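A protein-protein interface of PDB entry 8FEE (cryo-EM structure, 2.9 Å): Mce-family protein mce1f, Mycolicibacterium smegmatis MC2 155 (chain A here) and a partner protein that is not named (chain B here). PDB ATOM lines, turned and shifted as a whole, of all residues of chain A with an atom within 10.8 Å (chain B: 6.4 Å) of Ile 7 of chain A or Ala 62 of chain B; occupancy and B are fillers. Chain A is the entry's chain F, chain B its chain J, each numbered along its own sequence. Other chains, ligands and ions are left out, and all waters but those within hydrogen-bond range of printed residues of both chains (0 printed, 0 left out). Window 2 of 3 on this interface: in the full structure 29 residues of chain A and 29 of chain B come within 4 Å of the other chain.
The guanidinium group of Arg 59 of chain B lies within salt-bridge range of the side-chain carboxylate of Glu 63 of chain B (3.2 Å).
Printed residues of chain A that touch a printed residue of chain B: Leu 2, Ile 7, Gln 10 and Leu 11. Hydrophobic or aromatic side chains of chain A within 4 Å of the printed part of chain B: Leu 2, Ile 7 and Leu 11. Of the 11 printed residues of chain B, 5 touch a printed residue of chain A. Hydrophobic or aromatic side chains of chain B within 4 Å of the printed part of chain A: Val 61, Ala 62 and Met 66. Among the printed residues, 7 pairs touch across the chains. Among the printed residues, no Asp or Glu carboxylate lies within 4 Å of a Lys or Arg side-chain nitrogen of the other chain.
Leu 2 of chain A touches Arg 59 of chain B. Ile 7 of chain A touches Ala 62 of chain B (CG2 to CB, 3.7 Å). CD of Gln 10 of chain A touches CB of Met 66 of chain B, at 3.5 Å. CD1 of Leu 11 of chain A touches O of Leu 58 of chain B, at 3.8 Å. Val 61 of chain B touches Leu 11 of chain A (CG1 to CD1, 3.9 Å). Ala 62 of chain B touches Leu 11 of chain A (CB to CD1, 3.9 Å).
O of Ala 62 of chain B sits close to OE1 of Gln 10 of chain A (3.1 Å).
Ala 62 of chain B touches just these residues of chain A: Ile 7, Gln 10 and Leu 11. Of chain A, only Leu 11 (3.9 Å) comes within 4 Å of Val 61 of chain B. No residue of chain A comes within 4 Å of Gly 65 of chain B. Met 66 of chain B touches one residue of chain A. No residue of chain A comes within 4 Å of Gly 67 of chain B. Of the printed residues of chain B, Leu 2 of chain A touches Arg 59 (3.7 Å). Of the printed residues of chain A, Arg 59 of chain B touches Leu 2 (3.7 Å). The nearest printed residue of chain B that does not touch Leu 11 of chain A is Met 66 of chain B (5.7 Å).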
ATOM      1  N   MET A   1       4.831 -15.022  21.996  1.00  0.00           N
ATOM      2  CA  MET A   1       4.954 -16.364  22.551  1.00  0.00           C
ATOM      3  C   MET A   1       6.411 -16.812  22.511  1.00  0.00           C
ATOM      4  O   MET A   1       7.157 -16.430  21.607  1.00  0.00           O
ATOM      5  CB  MET A   1       4.063 -17.347  21.785  1.00  0.00           C
ATOM      6  CG  MET A   1       3.573 -18.539  22.602  1.00  0.00           C
ATOM      7  SD  MET A   1       4.834 -19.776  22.974  1.00  0.00           S
ATOM      8  CE  MET A   1       5.147 -20.439  21.340  1.00  0.00           C
ATOM      9  N   LEU A   2       6.799 -17.612  23.503  1.00  0.00           N
ATOM     10  CA  LEU A   2       8.151 -18.182  23.635  1.00  0.00           C
ATOM     11  C   LEU A   2       9.126 -17.012  23.771  1.00  0.00           C
ATOM     12  O   LEU A   2       8.890 -16.142  24.625  1.00  0.00           O
ATOM     13  CB  LEU A   2       8.419 -19.141  22.477  1.00  0.00           C
ATOM     14  CG  LEU A   2       9.595 -20.114  22.606  1.00  0.00           C
ATOM     15  CD1 LEU A   2       9.260 -21.244  23.568  1.00  0.00           C
ATOM     16  CD2 LEU A   2       9.990 -20.654  21.242  1.00  0.00           C
ATOM     17  N   LEU A   3      10.192 -16.946  22.969  1.00  0.00           N
ATOM     18  CA  LEU A   3      11.200 -15.884  23.032  1.00  0.00           C
ATOM     19  C   LEU A   3      11.782 -15.757  24.439  1.00  0.00           C
ATOM     20  O   LEU A   3      11.808 -14.679  25.037  1.00  0.00           O
ATOM     21  CB  LEU A   3      10.626 -14.552  22.545  1.00  0.00           C
ATOM     22  CG  LEU A   3      10.040 -14.556  21.131  1.00  0.00           C
ATOM     23  CD1 LEU A   3       9.537 -13.172  20.751  1.00  0.00           C
ATOM     24  CD2 LEU A   3      11.068 -15.052  20.126  1.00  0.00           C
ATOM     25  N   THR A   4      12.259 -16.883  24.966  1.00  0.00           N
ATOM     26  CA  THR A   4      12.797 -16.946  26.319  1.00  0.00           C
ATOM     27  C   THR A   4      14.207 -16.380  26.426  1.00  0.00           C
ATOM     28  O   THR A   4      14.753 -16.347  27.535  1.00  0.00           O
ATOM     29  CB  THR A   4      12.788 -18.390  26.825  1.00  0.00           C
ATOM     30  OG1 THR A   4      13.358 -18.442  28.138  1.00  0.00           O
ATOM     31  CG2 THR A   4      13.590 -19.282  25.897  1.00  0.00           C
ATOM     32  N   ARG A   5      14.813 -15.989  25.299  1.00  0.00           N
ATOM     33  CA  ARG A   5      16.163 -15.431  25.202  1.00  0.00           C
ATOM     34  C   ARG A   5      17.244 -16.458  25.524  1.00  0.00           C
ATOM     35  O   ARG A   5      18.437 -16.170  25.382  1.00  0.00           O
ATOM     36  CB  ARG A   5      16.319 -14.197  26.100  1.00  0.00           C
ATOM     37  CG  ARG A   5      15.317 -13.093  25.810  1.00  0.00           C
ATOM     38  CD  ARG A   5      15.855 -11.739  26.239  1.00  0.00           C
ATOM     39  NE  ARG A   5      17.137 -11.440  25.610  1.00  0.00           N
ATOM     40  CZ  ARG A   5      17.274 -10.944  24.388  1.00  0.00           C
ATOM     41  NH1 ARG A   5      16.223 -10.676  23.629  1.00  0.00           N
ATOM     42  NH2 ARG A   5      18.495 -10.711  23.916  1.00  0.00           N
ATOM     43  N   PHE A   6      16.847 -17.656  25.955  1.00  0.00           N
ATOM     44  CA  PHE A   6      17.771 -18.780  26.031  1.00  0.00           C
ATOM     45  C   PHE A   6      17.707 -19.638  24.776  1.00  0.00           C
ATOM     46  O   PHE A   6      18.738 -20.146  24.318  1.00  0.00           O
ATOM     47  CB  PHE A   6      17.466 -19.628  27.270  1.00  0.00           C
ATOM     48  CG  PHE A   6      18.207 -20.933  27.311  1.00  0.00           C
ATOM     49  CD1 PHE A   6      19.562 -20.966  27.592  1.00  0.00           C
ATOM     50  CD2 PHE A   6      17.546 -22.129  27.081  1.00  0.00           C
ATOM     51  CE1 PHE A   6      20.248 -22.165  27.634  1.00  0.00           C
ATOM     52  CE2 PHE A   6      18.225 -23.332  27.123  1.00  0.00           C
ATOM     53  CZ  PHE A   6      19.578 -23.349  27.400  1.00  0.00           C
ATOM     54  N   ILE A   7      16.510 -19.811  24.212  1.00  0.00           N
ATOM     55  CA  ILE A   7      16.382 -20.437  22.902  1.00  0.00           C
ATOM     56  C   ILE A   7      16.996 -19.553  21.823  1.00  0.00           C
ATOM     57  O   ILE A   7      17.595 -20.056  20.863  1.00  0.00           O
ATOM     58  CB  ILE A   7      14.899 -20.756  22.621  1.00  0.00           C
ATOM     59  CG1 ILE A   7      14.434 -21.926  23.491  1.00  0.00           C
ATOM     60  CG2 ILE A   7      14.661 -21.071  21.152  1.00  0.00           C
ATOM     61  CD1 ILE A   7      15.247 -23.187  23.303  1.00  0.00           C
ATOM     62  N   LYS A   8      16.882 -18.229  21.969  1.00  0.00           N
ATOM     63  CA  LYS A   8      17.444 -17.314  20.979  1.00  0.00           C
ATOM     64  C   LYS A   8      18.964 -17.415  20.930  1.00  0.00           C
ATOM     65  O   LYS A   8      19.566 -17.350  19.850  1.00  0.00           O
ATOM     66  CB  LYS A   8      17.010 -15.882  21.288  1.00  0.00           C
ATOM     67  CG  LYS A   8      17.161 -14.920  20.125  1.00  0.00           C
ATOM     68  CD  LYS A   8      16.241 -15.307  18.979  1.00  0.00           C
ATOM     69  CE  LYS A   8      16.385 -14.358  17.803  1.00  0.00           C
ATOM     70  NZ  LYS A   8      17.760 -14.379  17.237  1.00  0.00           N
ATOM     71  N   MET A   9      19.605 -17.558  22.095  1.00  0.00           N
ATOM     72  CA  MET A   9      21.052 -17.746  22.133  1.00  0.00           C
ATOM     73  C   MET A   9      21.457 -19.028  21.417  1.00  0.00           C
ATOM     74  O   MET A   9      22.432 -19.043  20.654  1.00  0.00           O
ATOM     75  CB  MET A   9      21.540 -17.763  23.581  1.00  0.00           C
ATOM     76  CG  MET A   9      22.982 -18.215  23.747  1.00  0.00           C
ATOM     77  SD  MET A   9      23.431 -18.507  25.468  1.00  0.00           S
ATOM     78  CE  MET A   9      25.115 -19.089  25.282  1.00  0.00           C
ATOM     79  N   GLN A  10      20.717 -20.114  21.654  1.00  0.00           N
ATOM     80  CA  GLN A  10      20.992 -21.363  20.954  1.00  0.00           C
ATOM     81  C   GLN A  10      20.826 -21.194  19.450  1.00  0.00           C
ATOM     82  O   GLN A  10      21.641 -21.694  18.666  1.00  0.00           O
ATOM     83  CB  GLN A  10      20.070 -22.465  21.475  1.00  0.00           C
ATOM     84  CG  GLN A  10      20.358 -22.896  22.902  1.00  0.00           C
ATOM     85  CD  GLN A  10      19.597 -24.147  23.290  1.00  0.00           C
ATOM     86  OE1 GLN A  10      18.738 -24.620  22.546  1.00  0.00           O
ATOM     87  NE2 GLN A  10      19.915 -24.697  24.456  1.00  0.00           N
ATOM     88  N   LEU A  11      19.780 -20.477  19.032  1.00  0.00           N
ATOM     89  CA  LEU A  11      19.535 -20.278  17.609  1.00  0.00           C
ATOM     90  C   LEU A  11      20.664 -19.487  16.956  1.00  0.00           C
ATOM     91  O   LEU A  11      21.142 -19.852  15.875  1.00  0.00           O
ATOM     92  CB  LEU A  11      18.195 -19.572  17.406  1.00  0.00           C
ATOM     93  CG  LEU A  11      17.305 -20.116  16.288  1.00  0.00           C
ATOM     94  CD1 LEU A  11      17.009 -21.589  16.514  1.00  0.00           C
ATOM     95  CD2 LEU A  11      16.017 -19.316  16.197  1.00  0.00           C
ATOM     96  N   VAL A  12      21.115 -18.408  17.604  1.00  0.00           N
ATOM     97  CA  VAL A  12      22.155 -17.584  16.993  1.00  0.00           C
ATOM     98  C   VAL A  12      23.495 -18.315  16.983  1.00  0.00           C
ATOM     99  O   VAL A  12      24.249 -18.225  16.005  1.00  0.00           O
ATOM    100  CB  VAL A  12      22.245 -16.199  17.668  1.00  0.00           C
ATOM    101  CG1 VAL A  12      20.931 -15.451  17.515  1.00  0.00           C
ATOM    102  CG2 VAL A  12      22.632 -16.297  19.133  1.00  0.00           C
ATOM    103  N   ILE A  13      23.820 -19.052  18.052  1.00  0.00           N
ATOM    104  CA  ILE A  13      25.086 -19.782  18.052  1.00  0.00           C
ATOM    105  C   ILE A  13      25.052 -20.899  17.013  1.00  0.00           C
ATOM    106  O   ILE A  13      26.058 -21.170  16.344  1.00  0.00           O
ATOM    107  CB  ILE A  13      25.442 -20.296  19.464  1.00  0.00           C
ATOM    108  CG1 ILE A  13      26.897 -20.774  19.502  1.00  0.00           C
ATOM    109  CG2 ILE A  13      24.528 -21.419  19.922  1.00  0.00           C
ATOM    110  CD1 ILE A  13      27.320 -21.346  20.839  1.00  0.00           C
ATOM    111  N   PHE A  14      23.893 -21.543  16.833  1.00  0.00           N
ATOM    112  CA  PHE A  14      23.777 -22.575  15.810  1.00  0.00           C
ATOM    113  C   PHE A  14      23.904 -21.982  14.413  1.00  0.00           C
ATOM    114  O   PHE A  14      24.527 -22.586  13.536  1.00  0.00           O
ATOM    115  CB  PHE A  14      22.454 -23.325  15.959  1.00  0.00           C
ATOM    116  CG  PHE A  14      22.263 -24.412  14.944  1.00  0.00           C
ATOM    117  CD1 PHE A  14      22.840 -25.656  15.128  1.00  0.00           C
ATOM    118  CD2 PHE A  14      21.506 -24.191  13.804  1.00  0.00           C
ATOM    119  CE1 PHE A  14      22.670 -26.657  14.196  1.00  0.00           C
ATOM    120  CE2 PHE A  14      21.332 -25.187  12.869  1.00  0.00           C
ATOM    121  CZ  PHE A  14      21.917 -26.422  13.064  1.00  0.00           C
ATOM    122  N   LEU A  15      23.318 -20.804  14.186  1.00  0.00           N
ATOM    123  CA  LEU A  15      23.441 -20.162  12.880  1.00  0.00           C
ATOM    124  C   LEU A  15      24.885 -19.766  12.594  1.00  0.00           C
ATOM    125  O   LEU A  15      25.371 -19.933  11.466  1.00  0.00           O
ATOM    126  CB  LEU A  15      22.524 -18.944  12.803  1.00  0.00           C
ATOM    127  CG  LEU A  15      22.414 -18.288  11.426  1.00  0.00           C
ATOM    128  CD1 LEU A  15      21.746 -19.234  10.441  1.00  0.00           C
ATOM    129  CD2 LEU A  15      21.654 -16.975  11.513  1.00  0.00           C
ATOM    130  N   LEU A  17      27.586 -21.219  13.856  1.00  0.00           N
ATOM    131  CA  LEU A  17      28.306 -22.464  13.607  1.00  0.00           C
ATOM    132  C   LEU A  17      28.019 -22.987  12.206  1.00  0.00           C
ATOM    133  O   LEU A  17      28.927 -23.460  11.513  1.00  0.00           O
ATOM    134  CB  LEU A  17      27.931 -23.505  14.660  1.00  0.00           C
ATOM    135  CG  LEU A  17      28.955 -24.606  14.942  1.00  0.00           C
ATOM    136  CD1 LEU A  17      30.266 -24.009  15.425  1.00  0.00           C
ATOM    137  CD2 LEU A  17      28.410 -25.597  15.956  1.00  0.00           C
ATOM    138  N   THR A  18      26.760 -22.895  11.770  1.00  0.00           N
ATOM    139  CA  THR A  18      26.381 -23.333  10.432  1.00  0.00           C
ATOM    140  C   THR A  18      27.123 -22.543   9.365  1.00  0.00           C
ATOM    141  O   THR A  18      27.685 -23.119   8.427  1.00  0.00           O
ATOM    142  CB  THR A  18      24.872 -23.175  10.245  1.00  0.00           C
ATOM    143  OG1 THR A  18      24.178 -24.041  11.150  1.00  0.00           O
ATOM    144  CG2 THR A  18      24.473 -23.491   8.811  1.00  0.00           C
ATOM    145  N   SER B  57       8.528 -24.569  15.532  1.00  0.00           N
ATOM    146  CA  SER B  57       9.619 -25.047  14.690  1.00  0.00           C
ATOM    147  C   SER B  57      10.956 -24.475  15.138  1.00  0.00           C
ATOM    148  O   SER B  57      11.959 -25.192  15.174  1.00  0.00           O
ATOM    149  CB  SER B  57       9.349 -24.695  13.228  1.00  0.00           C
ATOM    150  OG  SER B  57       8.252 -25.434  12.720  1.00  0.00           O
ATOM    151  N   LEU B  58      10.993 -23.186  15.485  1.00  0.00           N
ATOM    152  CA  LEU B  58      12.243 -22.592  15.952  1.00  0.00           C
ATOM    153  C   LEU B  58      12.685 -23.203  17.277  1.00  0.00           C
ATOM    154  O   LEU B  58      13.880 -23.467  17.480  1.00  0.00           O
ATOM    155  CB  LEU B  58      12.092 -21.077  16.081  1.00  0.00           C
ATOM    156  CG  LEU B  58      11.810 -20.315  14.785  1.00  0.00           C
ATOM    157  CD1 LEU B  58      11.877 -18.815  15.019  1.00  0.00           C
ATOM    158  CD2 LEU B  58      12.776 -20.738  13.691  1.00  0.00           C
ATOM    159  N   ARG B  59      11.738 -23.435  18.191  1.00  0.00           N
ATOM    160  CA  ARG B  59      12.076 -24.069  19.462  1.00  0.00           C
ATOM    161  C   ARG B  59      12.618 -25.478  19.251  1.00  0.00           C
ATOM    162  O   ARG B  59      13.608 -25.870  19.880  1.00  0.00           O
ATOM    163  CB  ARG B  59      10.856 -24.099  20.380  1.00  0.00           C
ATOM    164  CG  ARG B  59      11.162 -24.582  21.789  1.00  0.00           C
ATOM    165  CD  ARG B  59       9.893 -24.822  22.588  1.00  0.00           C
ATOM    166  NE  ARG B  59       9.063 -25.867  22.004  1.00  0.00           N
ATOM    167  CZ  ARG B  59       9.227 -27.164  22.224  1.00  0.00           C
ATOM    168  NH1 ARG B  59      10.199 -27.616  22.999  1.00  0.00           N
ATOM    169  NH2 ARG B  59       8.395 -28.029  21.653  1.00  0.00           N
ATOM    170  N   LEU B  60      11.990 -26.252  18.363  1.00  0.00           N
ATOM    171  CA  LEU B  60      12.480 -27.599  18.090  1.00  0.00           C
ATOM    172  C   LEU B  60      13.834 -27.573  17.392  1.00  0.00           C
ATOM    173  O   LEU B  60      14.674 -28.444  17.637  1.00  0.00           O
ATOM    174  CB  LEU B  60      11.459 -28.379  17.265  1.00  0.00           C
ATOM    175  CG  LEU B  60      10.199 -28.772  18.034  1.00  0.00           C
ATOM    176  CD1 LEU B  60       9.381 -29.777  17.250  1.00  0.00           C
ATOM    177  CD2 LEU B  60      10.562 -29.326  19.399  1.00  0.00           C
ATOM    178  N   VAL B  61      14.068 -26.588  16.522  1.00  0.00           N
ATOM    179  CA  VAL B  61      15.368 -26.463  15.866  1.00  0.00           C
ATOM    180  C   VAL B  61      16.454 -26.199  16.900  1.00  0.00           C
ATOM    181  O   VAL B  61      17.520 -26.825  16.881  1.00  0.00           O
ATOM    182  CB  VAL B  61      15.328 -25.362  14.791  1.00  0.00           C
ATOM    183  CG1 VAL B  61      16.730 -24.874  14.467  1.00  0.00           C
ATOM    184  CG2 VAL B  61      14.652 -25.877  13.534  1.00  0.00           C
ATOM    185  N   ALA B  62      16.191 -25.274  17.828  1.00  0.00           N
ATOM    186  CA  ALA B  62      17.157 -25.001  18.887  1.00  0.00           C
ATOM    187  C   ALA B  62      17.383 -26.231  19.761  1.00  0.00           C
ATOM    188  O   ALA B  62      18.526 -26.548  20.117  1.00  0.00           O
ATOM    189  CB  ALA B  62      16.690 -23.819  19.735  1.00  0.00           C
ATOM    190  N   GLU B  63      16.304 -26.941  20.105  1.00  0.00           N
ATOM    191  CA  GLU B  63      16.424 -28.124  20.952  1.00  0.00           C
ATOM    192  C   GLU B  63      17.249 -29.211  20.275  1.00  0.00           C
ATOM    193  O   GLU B  63      18.099 -29.842  20.912  1.00  0.00           O
ATOM    194  CB  GLU B  63      15.034 -28.649  21.314  1.00  0.00           C
ATOM    195  CG  GLU B  63      15.035 -29.962  22.078  1.00  0.00           C
ATOM    196  CD  GLU B  63      13.655 -30.345  22.576  1.00  0.00           C
ATOM    197  OE1 GLU B  63      12.739 -29.500  22.500  1.00  0.00           O
ATOM    198  OE2 GLU B  63      13.485 -31.491  23.042  1.00  0.00           O
ATOM    199  N   ILE B  64      17.012 -29.447  18.984  1.00  0.00           N
ATOM    200  CA  ILE B  64      17.739 -30.494  18.274  1.00  0.00           C
ATOM    201  C   ILE B  64      19.196 -30.093  18.075  1.00  0.00           C
ATOM    202  O   ILE B  64      20.106 -30.916  18.228  1.00  0.00           O
ATOM    203  CB  ILE B  64      17.042 -30.815  16.939  1.00  0.00           C
ATOM    204  CG1 ILE B  64      15.662 -31.425  17.194  1.00  0.00           C
ATOM    205  CG2 ILE B  64      17.888 -31.749  16.096  1.00  0.00           C
ATOM    206  CD1 ILE B  64      14.934 -31.844  15.939  1.00  0.00           C
ATOM    207  N   GLY B  65      19.448 -28.823  17.749  1.00  0.00           N
ATOM    208  CA  GLY B  65      20.811 -28.386  17.519  1.00  0.00           C
ATOM    209  C   GLY B  65      21.648 -28.269  18.774  1.00  0.00           C
ATOM    210  O   GLY B  65      22.878 -28.327  18.690  1.00  0.00           O
ATOM    211  N   MET B  66      21.014 -28.104  19.937  1.00  0.00           N
ATOM    212  CA  MET B  66      21.751 -27.945  21.186  1.00  0.00           C
ATOM    213  C   MET B  66      21.372 -28.994  22.226  1.00  0.00           C
ATOM    214  O   MET B  66      21.683 -28.827  23.410  1.00  0.00           O
ATOM    215  CB  MET B  66      21.552 -26.538  21.747  1.00  0.00           C
ATOM    216  CG  MET B  66      22.014 -25.435  20.809  1.00  0.00           C
ATOM    217  SD  MET B  66      23.736 -25.616  20.302  1.00  0.00           S
ATOM    218  CE  MET B  66      24.565 -25.595  21.890  1.00  0.00           C
ATOM    219  N   GLY B  67      20.710 -30.070  21.812  1.00  0.00           N
ATOM    220  CA  GLY B  67      20.415 -31.172  22.709  1.00  0.00           C
ATOM    221  C   GLY B  67      19.387 -30.808  23.771  1.00  0.00           C
ATOM    222  O   GLY B  67      18.847 -29.706  23.821  1.00  0.00           O
